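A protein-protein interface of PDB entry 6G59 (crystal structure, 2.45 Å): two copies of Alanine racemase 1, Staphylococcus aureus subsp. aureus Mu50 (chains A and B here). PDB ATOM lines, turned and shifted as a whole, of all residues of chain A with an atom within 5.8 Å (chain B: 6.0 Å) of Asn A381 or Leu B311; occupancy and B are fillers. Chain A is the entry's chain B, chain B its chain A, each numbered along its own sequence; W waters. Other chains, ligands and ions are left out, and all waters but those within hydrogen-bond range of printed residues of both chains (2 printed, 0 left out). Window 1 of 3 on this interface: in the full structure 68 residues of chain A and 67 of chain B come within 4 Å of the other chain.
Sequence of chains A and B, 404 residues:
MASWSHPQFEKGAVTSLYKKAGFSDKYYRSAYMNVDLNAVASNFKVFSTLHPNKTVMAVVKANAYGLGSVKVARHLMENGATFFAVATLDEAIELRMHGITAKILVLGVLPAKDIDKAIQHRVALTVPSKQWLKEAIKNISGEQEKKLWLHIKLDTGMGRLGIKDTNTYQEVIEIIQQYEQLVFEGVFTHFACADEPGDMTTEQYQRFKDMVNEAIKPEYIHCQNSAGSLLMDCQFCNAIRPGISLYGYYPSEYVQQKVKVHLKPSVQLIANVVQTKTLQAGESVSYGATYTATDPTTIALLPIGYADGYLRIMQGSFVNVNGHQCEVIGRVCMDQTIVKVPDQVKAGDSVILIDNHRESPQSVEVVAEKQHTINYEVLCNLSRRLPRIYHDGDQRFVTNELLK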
ATOM      1  N   ASP A 308      -4.212   1.232  23.876  1.00  0.00           N
ATOM      2  CA  ASP A 308      -4.726  -0.069  23.424  1.00  0.00           C
ATOM      3  C   ASP A 308      -6.211  -0.258  23.709  1.00  0.00           C
ATOM      4  O   ASP A 308      -6.814  -1.248  23.264  1.00  0.00           O
ATOM      5  CB  ASP A 308      -3.911  -1.204  24.077  1.00  0.00           C
ATOM      6  CG  ASP A 308      -2.424  -1.081  23.779  1.00  0.00           C
ATOM      7  OD1 ASP A 308      -2.067  -1.205  22.589  1.00  0.00           O
ATOM      8  OD2 ASP A 308      -1.610  -0.841  24.697  1.00  0.00           O
ATOM      9  N   GLY A 309      -6.807   0.678  24.430  1.00  0.00           N
ATOM     10  CA  GLY A 309      -8.213   0.563  24.841  1.00  0.00           C
ATOM     11  C   GLY A 309      -8.446   0.116  26.273  1.00  0.00           C
ATOM     12  O   GLY A 309      -9.600   0.024  26.681  1.00  0.00           O
ATOM     13  N   TYR A 310      -7.370  -0.170  27.025  1.00  0.00           N
ATOM     14  CA  TYR A 310      -7.467  -0.476  28.464  1.00  0.00           C
ATOM     15  C   TYR A 310      -7.352   0.855  29.204  1.00  0.00           C
ATOM     16  O   TYR A 310      -6.255   1.271  29.612  1.00  0.00           O
ATOM     17  CB  TYR A 310      -6.403  -1.499  28.902  1.00  0.00           C
ATOM     18  CG  TYR A 310      -6.734  -2.201  30.217  1.00  0.00           C
ATOM     19  CD1 TYR A 310      -7.761  -3.153  30.280  1.00  0.00           C
ATOM     20  CD2 TYR A 310      -6.016  -1.922  31.400  1.00  0.00           C
ATOM     21  CE1 TYR A 310      -8.078  -3.795  31.461  1.00  0.00           C
ATOM     22  CE2 TYR A 310      -6.333  -2.561  32.586  1.00  0.00           C
ATOM     23  CZ  TYR A 310      -7.364  -3.501  32.612  1.00  0.00           C
ATOM     24  OH  TYR A 310      -7.689  -4.147  33.789  1.00  0.00           O
ATOM     25  N   LEU A 311      -8.511   1.502  29.373  1.00  0.00           N
ATOM     26  CA  LEU A 311      -8.583   2.926  29.710  1.00  0.00           C
ATOM     27  C   LEU A 311      -8.126   3.231  31.137  1.00  0.00           C
ATOM     28  O   LEU A 311      -8.019   2.336  31.985  1.00  0.00           O
ATOM     29  CB  LEU A 311      -9.998   3.480  29.476  1.00  0.00           C
ATOM     30  CG  LEU A 311     -10.645   3.320  28.086  1.00  0.00           C
ATOM     31  CD1 LEU A 311     -11.987   4.046  28.066  1.00  0.00           C
ATOM     32  CD2 LEU A 311      -9.758   3.794  26.915  1.00  0.00           C
ATOM     33  N   GLN A 371     -15.791   0.747  33.680  1.00  0.00           N
ATOM     34  CA  GLN A 371     -15.749   1.871  32.736  1.00  0.00           C
ATOM     35  C   GLN A 371     -17.025   2.722  32.737  1.00  0.00           C
ATOM     36  O   GLN A 371     -17.090   3.702  31.986  1.00  0.00           O
ATOM     37  CB  GLN A 371     -15.477   1.362  31.316  1.00  0.00           C
ATOM     38  CG  GLN A 371     -14.098   0.743  31.129  1.00  0.00           C
ATOM     39  CD  GLN A 371     -13.793   0.374  29.685  1.00  0.00           C
ATOM     40  OE1 GLN A 371     -14.443   0.874  28.752  1.00  0.00           O
ATOM     41  NE2 GLN A 371     -12.810  -0.499  29.490  1.00  0.00           N
ATOM     42  N   THR A 373     -19.974   2.003  31.563  1.00  0.00           N
ATOM     43  CA  THR A 373     -20.489   1.933  30.191  1.00  0.00           C
ATOM     44  C   THR A 373     -21.154   0.553  29.950  1.00  0.00           C
ATOM     45  O   THR A 373     -21.494  -0.137  30.891  1.00  0.00           O
ATOM     46  CB  THR A 373     -19.355   2.270  29.157  1.00  0.00           C
ATOM     47  OG1 THR A 373     -19.910   2.556  27.864  1.00  0.00           O
ATOM     48  CG2 THR A 373     -18.359   1.120  28.999  1.00  0.00           C
ATOM     49  N   TYR A 376     -20.742  -3.274  24.670  1.00  0.00           N
ATOM     50  CA  TYR A 376     -20.514  -2.800  23.294  1.00  0.00           C
ATOM     51  C   TYR A 376     -19.291  -1.860  23.188  1.00  0.00           C
ATOM     52  O   TYR A 376     -18.464  -1.984  22.284  1.00  0.00           O
ATOM     53  CB  TYR A 376     -21.731  -2.003  22.784  1.00  0.00           C
ATOM     54  CG  TYR A 376     -23.077  -2.722  22.617  1.00  0.00           C
ATOM     55  CD1 TYR A 376     -23.983  -2.853  23.679  1.00  0.00           C
ATOM     56  CD2 TYR A 376     -23.475  -3.191  21.381  1.00  0.00           C
ATOM     57  CE1 TYR A 376     -25.207  -3.496  23.505  1.00  0.00           C
ATOM     58  CE2 TYR A 376     -24.693  -3.816  21.193  1.00  0.00           C
ATOM     59  CZ  TYR A 376     -25.554  -3.972  22.248  1.00  0.00           C
ATOM     60  OH  TYR A 376     -26.758  -4.600  22.033  1.00  0.00           O
ATOM     61  N   GLU A 377     -19.202  -0.910  24.115  1.00  0.00           N
ATOM     62  CA  GLU A 377     -18.133   0.100  24.094  1.00  0.00           C
ATOM     63  C   GLU A 377     -16.793  -0.458  24.543  1.00  0.00           C
ATOM     64  O   GLU A 377     -15.763  -0.039  24.010  1.00  0.00           O
ATOM     65  CB  GLU A 377     -18.500   1.323  24.947  1.00  0.00           C
ATOM     66  CG  GLU A 377     -17.482   2.470  24.903  1.00  0.00           C
ATOM     67  CD  GLU A 377     -18.026   3.770  25.490  1.00  0.00           C
ATOM     68  OE1 GLU A 377     -17.989   3.962  26.736  1.00  0.00           O
ATOM     69  OE2 GLU A 377     -18.481   4.613  24.680  1.00  0.00           O
ATOM     70  N   VAL A 378     -16.791  -1.393  25.506  1.00  0.00           N
ATOM     71  CA  VAL A 378     -15.537  -2.041  25.935  1.00  0.00           C
ATOM     72  C   VAL A 378     -14.803  -2.687  24.751  1.00  0.00           C
ATOM     73  O   VAL A 378     -13.574  -2.556  24.618  1.00  0.00           O
ATOM     74  CB  VAL A 378     -15.757  -3.108  27.031  1.00  0.00           C
ATOM     75  CG1 VAL A 378     -14.480  -3.921  27.288  1.00  0.00           C
ATOM     76  CG2 VAL A 378     -16.221  -2.453  28.320  1.00  0.00           C
ATOM     77  N   LEU A 379     -15.575  -3.362  23.901  1.00  0.00           N
ATOM     78  CA  LEU A 379     -15.050  -4.023  22.719  1.00  0.00           C
ATOM     79  C   LEU A 379     -14.607  -3.059  21.632  1.00  0.00           C
ATOM     80  O   LEU A 379     -13.574  -3.268  21.030  1.00  0.00           O
ATOM     81  CB  LEU A 379     -16.107  -4.967  22.156  1.00  0.00           C
ATOM     82  CG  LEU A 379     -16.537  -6.097  23.079  1.00  0.00           C
ATOM     83  CD1 LEU A 379     -17.830  -6.727  22.568  1.00  0.00           C
ATOM     84  CD2 LEU A 379     -15.414  -7.121  23.212  1.00  0.00           C
ATOM     85  N   CYS A 380     -15.395  -2.017  21.369  1.00  0.00           N
ATOM     86  CA  CYS A 380     -15.062  -1.005  20.350  1.00  0.00           C
ATOM     87  C   CYS A 380     -13.826  -0.148  20.692  1.00  0.00           C
ATOM     88  O   CYS A 380     -13.129   0.310  19.777  1.00  0.00           O
ATOM     89  CB  CYS A 380     -16.260  -0.083  20.084  1.00  0.00           C
ATOM     90  SG  CYS A 380     -17.663  -0.893  19.267  1.00  0.00           S
ATOM     91  N   ASN A 381     -13.568   0.059  21.992  1.00  0.00           N
ATOM     92  CA  ASN A 381     -12.366   0.747  22.474  1.00  0.00           C
ATOM     93  C   ASN A 381     -11.039   0.065  22.090  1.00  0.00           C
ATOM     94  O   ASN A 381      -9.984   0.728  22.029  1.00  0.00           O
ATOM     95  CB  ASN A 381     -12.391   0.867  23.999  1.00  0.00           C
ATOM     96  CG  ASN A 381     -13.359   1.918  24.516  1.00  0.00           C
ATOM     97  OD1 ASN A 381     -13.733   2.850  23.815  1.00  0.00           O
ATOM     98  ND2 ASN A 381     -13.749   1.776  25.781  1.00  0.00           N
ATOM     99  N   LEU A 382     -11.075  -1.249  21.863  1.00  0.00           N
ATOM    100  CA  LEU A 382      -9.853  -2.012  21.626  1.00  0.00           C
ATOM    101  C   LEU A 382      -9.194  -1.574  20.299  1.00  0.00           C
ATOM    102  O   LEU A 382      -9.757  -1.766  19.237  1.00  0.00           O
ATOM    103  CB  LEU A 382     -10.125  -3.521  21.691  1.00  0.00           C
ATOM    104  CG  LEU A 382     -10.652  -4.034  23.044  1.00  0.00           C
ATOM    105  CD1 LEU A 382     -10.943  -5.531  22.982  1.00  0.00           C
ATOM    106  CD2 LEU A 382      -9.709  -3.749  24.196  1.00  0.00           C
ATOM    107  N   SER A 383      -8.001  -0.969  20.402  1.00  0.00           N
ATOM    108  CA  SER A 383      -7.426  -0.192  19.304  1.00  0.00           C
ATOM    109  C   SER A 383      -6.699  -1.047  18.270  1.00  0.00           C
ATOM    110  O   SER A 383      -6.485  -2.253  18.457  1.00  0.00           O
ATOM    111  CB  SER A 383      -6.496   0.917  19.843  1.00  0.00           C
ATOM    112  OG  SER A 383      -5.162   0.469  20.072  1.00  0.00           O
ATOM    113  N   GLY B 305     -20.125   8.126  16.250  1.00  0.00           N
ATOM    114  CA  GLY B 305     -20.565   7.513  17.505  1.00  0.00           C
ATOM    115  C   GLY B 305     -19.397   7.003  18.307  1.00  0.00           C
ATOM    116  O   GLY B 305     -18.248   7.394  18.052  1.00  0.00           O
ATOM    117  N   TYR B 306     -19.676   6.127  19.274  1.00  0.00           N
ATOM    118  CA  TYR B 306     -18.624   5.691  20.208  1.00  0.00           C
ATOM    119  C   TYR B 306     -17.633   4.699  19.625  1.00  0.00           C
ATOM    120  O   TYR B 306     -16.525   4.591  20.141  1.00  0.00           O
ATOM    121  CB  TYR B 306     -19.192   5.200  21.555  1.00  0.00           C
ATOM    122  CG  TYR B 306     -20.128   4.003  21.545  1.00  0.00           C
ATOM    123  CD1 TYR B 306     -19.636   2.702  21.463  1.00  0.00           C
ATOM    124  CD2 TYR B 306     -21.496   4.173  21.692  1.00  0.00           C
ATOM    125  CE1 TYR B 306     -20.497   1.601  21.503  1.00  0.00           C
ATOM    126  CE2 TYR B 306     -22.362   3.084  21.731  1.00  0.00           C
ATOM    127  CZ  TYR B 306     -21.857   1.797  21.633  1.00  0.00           C
ATOM    128  OH  TYR B 306     -22.709   0.732  21.663  1.00  0.00           O
ATOM    129  N   GLY B 309     -14.738   6.721  18.787  1.00  0.00           N
ATOM    130  CA  GLY B 309     -14.056   7.353  19.918  1.00  0.00           C
ATOM    131  C   GLY B 309     -14.806   8.502  20.562  1.00  0.00           C
ATOM    132  O   GLY B 309     -14.300   9.067  21.530  1.00  0.00           O
ATOM    133  N   TYR B 310     -15.987   8.864  20.034  1.00  0.00           N
ATOM    134  CA  TYR B 310     -16.861   9.861  20.661  1.00  0.00           C
ATOM    135  C   TYR B 310     -17.778   9.106  21.619  1.00  0.00           C
ATOM    136  O   TYR B 310     -18.902   8.713  21.262  1.00  0.00           O
ATOM    137  CB  TYR B 310     -17.644  10.675  19.612  1.00  0.00           C
ATOM    138  CG  TYR B 310     -18.177  12.007  20.145  1.00  0.00           C
ATOM    139  CD1 TYR B 310     -17.309  13.066  20.416  1.00  0.00           C
ATOM    140  CD2 TYR B 310     -19.541  12.207  20.374  1.00  0.00           C
ATOM    141  CE1 TYR B 310     -17.778  14.268  20.905  1.00  0.00           C
ATOM    142  CE2 TYR B 310     -20.014  13.411  20.870  1.00  0.00           C
ATOM    143  CZ  TYR B 310     -19.125  14.435  21.134  1.00  0.00           C
ATOM    144  OH  TYR B 310     -19.568  15.645  21.626  1.00  0.00           O
ATOM    145  N   LEU B 311     -17.267   8.914  22.842  1.00  0.00           N
ATOM    146  CA  LEU B 311     -17.780   7.921  23.782  1.00  0.00           C
ATOM    147  C   LEU B 311     -19.160   8.268  24.338  1.00  0.00           C
ATOM    148  O   LEU B 311     -19.625   9.406  24.235  1.00  0.00           O
ATOM    149  CB  LEU B 311     -16.787   7.688  24.935  1.00  0.00           C
ATOM    150  CG  LEU B 311     -15.337   7.276  24.612  1.00  0.00           C
ATOM    151  CD1 LEU B 311     -14.578   6.946  25.895  1.00  0.00           C
ATOM    152  CD2 LEU B 311     -15.236   6.088  23.661  1.00  0.00           C
ATOM    153  N   ARG B 312     -19.810   7.269  24.929  1.00  0.00           N
ATOM    154  CA  ARG B 312     -21.185   7.410  25.413  1.00  0.00           C
ATOM    155  C   ARG B 312     -21.346   8.528  26.422  1.00  0.00           C
ATOM    156  O   ARG B 312     -22.360   9.213  26.422  1.00  0.00           O
ATOM    157  CB  ARG B 312     -21.694   6.091  26.006  1.00  0.00           C
ATOM    158  CG  ARG B 312     -21.996   5.075  24.912  1.00  0.00           C
ATOM    159  CD  ARG B 312     -22.299   3.699  25.469  1.00  0.00           C
ATOM    160  NE  ARG B 312     -23.675   3.595  25.952  1.00  0.00           N
ATOM    161  CZ  ARG B 312     -24.065   3.590  27.225  1.00  0.00           C
ATOM    162  NH1 ARG B 312     -23.201   3.710  28.226  1.00  0.00           N
ATOM    163  NH2 ARG B 312     -25.356   3.475  27.495  1.00  0.00           N
ATOM    164  N   ILE B 313     -20.329   8.718  27.260  1.00  0.00           N
ATOM    165  CA  ILE B 313     -20.327   9.770  28.270  1.00  0.00           C
ATOM    166  C   ILE B 313     -20.409  11.190  27.673  1.00  0.00           C
ATOM    167  O   ILE B 313     -20.706  12.135  28.389  1.00  0.00           O
ATOM    168  CB  ILE B 313     -19.095   9.628  29.203  1.00  0.00           C
ATOM    169  CG1 ILE B 313     -19.282  10.425  30.498  1.00  0.00           C
ATOM    170  CG2 ILE B 313     -17.802  10.025  28.495  1.00  0.00           C
ATOM    171  CD1 ILE B 313     -18.174  10.180  31.511  1.00  0.00           C
ATOM    172  N   MET B 314     -20.172  11.348  26.371  1.00  0.00           N
ATOM    173  CA  MET B 314     -20.320  12.657  25.731  1.00  0.00           C
ATOM    174  C   MET B 314     -21.754  13.173  25.682  1.00  0.00           C
ATOM    175  O   MET B 314     -21.955  14.325  25.322  1.00  0.00           O
ATOM    176  CB  MET B 314     -19.725  12.661  24.310  1.00  0.00           C
ATOM    177  CG  MET B 314     -18.223  12.369  24.228  1.00  0.00           C
ATOM    178  SD  MET B 314     -17.208  13.387  25.295  1.00  0.00           S
ATOM    179  CE  MET B 314     -17.373  14.977  24.494  1.00  0.00           C
ATOM    180  N   GLN B 315     -22.742  12.340  26.016  1.00  0.00           N
ATOM    181  CA  GLN B 315     -24.139  12.781  26.160  1.00  0.00           C
ATOM    182  C   GLN B 315     -24.203  13.937  27.159  1.00  0.00           C
ATOM    183  O   GLN B 315     -23.617  13.862  28.238  1.00  0.00           O
ATOM    184  CB  GLN B 315     -25.052  11.621  26.593  1.00  0.00           C
ATOM    185  CG  GLN B 315     -26.519  11.979  26.723  1.00  0.00           C
ATOM    186  CD  GLN B 315     -27.417  10.775  27.053  1.00  0.00           C
ATOM    187  OE1 GLN B 315     -26.948   9.621  27.135  1.00  0.00           O
ATOM    188  NE2 GLN B 315     -28.718  11.041  27.226  1.00  0.00           N
ATOM    189  N   VAL B 332     -25.660   8.290  22.908  1.00  0.00           N
ATOM    190  CA  VAL B 332     -24.722   8.227  21.810  1.00  0.00           C
ATOM    191  C   VAL B 332     -24.679   6.749  21.404  1.00  0.00           C
ATOM    192  O   VAL B 332     -24.448   5.879  22.236  1.00  0.00           O
ATOM    193  CB  VAL B 332     -23.320   8.708  22.203  1.00  0.00           C
ATOM    194  CG1 VAL B 332     -22.365   8.596  21.023  1.00  0.00           C
ATOM    195  CG2 VAL B 332     -23.364  10.141  22.714  1.00  0.00           C
ATOM    196  N   GLN B 371     -15.202  13.428  29.697  1.00  0.00           N
ATOM    197  CA  GLN B 371     -14.845  12.017  29.776  1.00  0.00           C
ATOM    198  C   GLN B 371     -14.174  11.614  31.086  1.00  0.00           C
ATOM    199  O   GLN B 371     -13.825  10.434  31.246  1.00  0.00           O
ATOM    200  CB  GLN B 371     -13.923  11.641  28.605  1.00  0.00           C
ATOM    201  CG  GLN B 371     -14.577  11.711  27.238  1.00  0.00           C
ATOM    202  CD  GLN B 371     -13.659  11.240  26.123  1.00  0.00           C
ATOM    203  OE1 GLN B 371     -12.682  10.519  26.367  1.00  0.00           O
ATOM    204  NE2 GLN B 371     -13.969  11.649  24.879  1.00  0.00           N
ATOM    205  N   ASN B 381      -8.287   7.566  21.938  1.00  0.00           N
ATOM    206  CA  ASN B 381      -9.615   6.974  21.684  1.00  0.00           C
ATOM    207  C   ASN B 381     -10.085   7.045  20.224  1.00  0.00           C
ATOM    208  O   ASN B 381     -10.917   6.237  19.800  1.00  0.00           O
ATOM    209  CB  ASN B 381     -10.693   7.673  22.531  1.00  0.00           C
ATOM    210  CG  ASN B 381     -10.657   7.280  23.993  1.00  0.00           C
ATOM    211  OD1 ASN B 381     -10.118   6.222  24.377  1.00  0.00           O
ATOM    212  ND2 ASN B 381     -11.247   8.135  24.827  1.00  0.00           N
HETATM  213  O   HOH W   1     -20.862   5.256  29.362  1.00  0.00           O
HETATM  214  O   HOH W   2     -18.648   6.507  27.895  1.00  0.00           O
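The side-chain carboxylate (OE2) of Glu A377 sits at hydrogen-bond distance from the backbone NH (N) of Arg B312.
The side-chain amide oxygen of Gln B371 sits at hydrogen-bond distance from the side-chain amide nitrogen of Asn B381 (3.2 Å). The side-chain amide oxygen (OE1) of Gln A371 lies within hydrogen-bond range of the side-chain amide nitrogen (ND2) of Asn A381 (3.2 Å). OE1 of Glu A377 is in hydrogen-bond range of OG1 of Thr A373, 2.6 Å away. The side-chain sulfur of Cys A380 lies within hydrogen-bond range of the backbone carbonyl oxygen of Tyr A376 (3.3 Å). ND2 of Asn A381 sits close to O of Glu A377 (3.2 Å).
Among the printed residues, merely in contact across the chains: Tyr A376 with Tyr B306 (3.1 Å), Glu A377 with Tyr B306 (3.3 Å), Glu A377 with Leu B311 (3.5 Å), Thr A373 with Arg B312 (3.5 Å), Leu A311 with Asn B381 (3.5 Å) and Asn A381 with Leu B311 (3.6 Å).
Of the printed residues of chain B, Leu A311 touches Asn B381 (3.5 Å). Of the printed residues of chain B, Tyr A376 touches Tyr B306 (3.1 Å). Of chain B, only Leu B311 comes within 4 Å of Asn A381. Leu B311 touches two residues of chain A. Ile B313 touches none of the printed residues of chain A. Gln B371 touches none of the printed residues of chain A. The nearest residue of chain B that does not touch Asn A381 is Tyr B306 (4.9 Å).
Hydrophobic or aromatic side chains of chain A that line the printed part of chain B: Leu A311 and Tyr A376.
Leu A311 touches Asn B381, and with the chains exchanged Asn A381 touches Leu B311. Positions printed for both chains: 309, 310, 311, 371 and 381. Of the 7 pairs that touch across the chains among the printed residues, 2 have their exchanged pair printed and touching as well.
Water W2 lies within hydrogen-bond range of N of Ile B313 (2.8 Å), OE1 of Glu A377 (2.9 Å) and N of Arg B312 (3.3 Å). Water W1 lies within hydrogen-bond range of NH1 of Arg B312 (3.0 Å) and OG1 of Thr A373 (3.2 Å).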
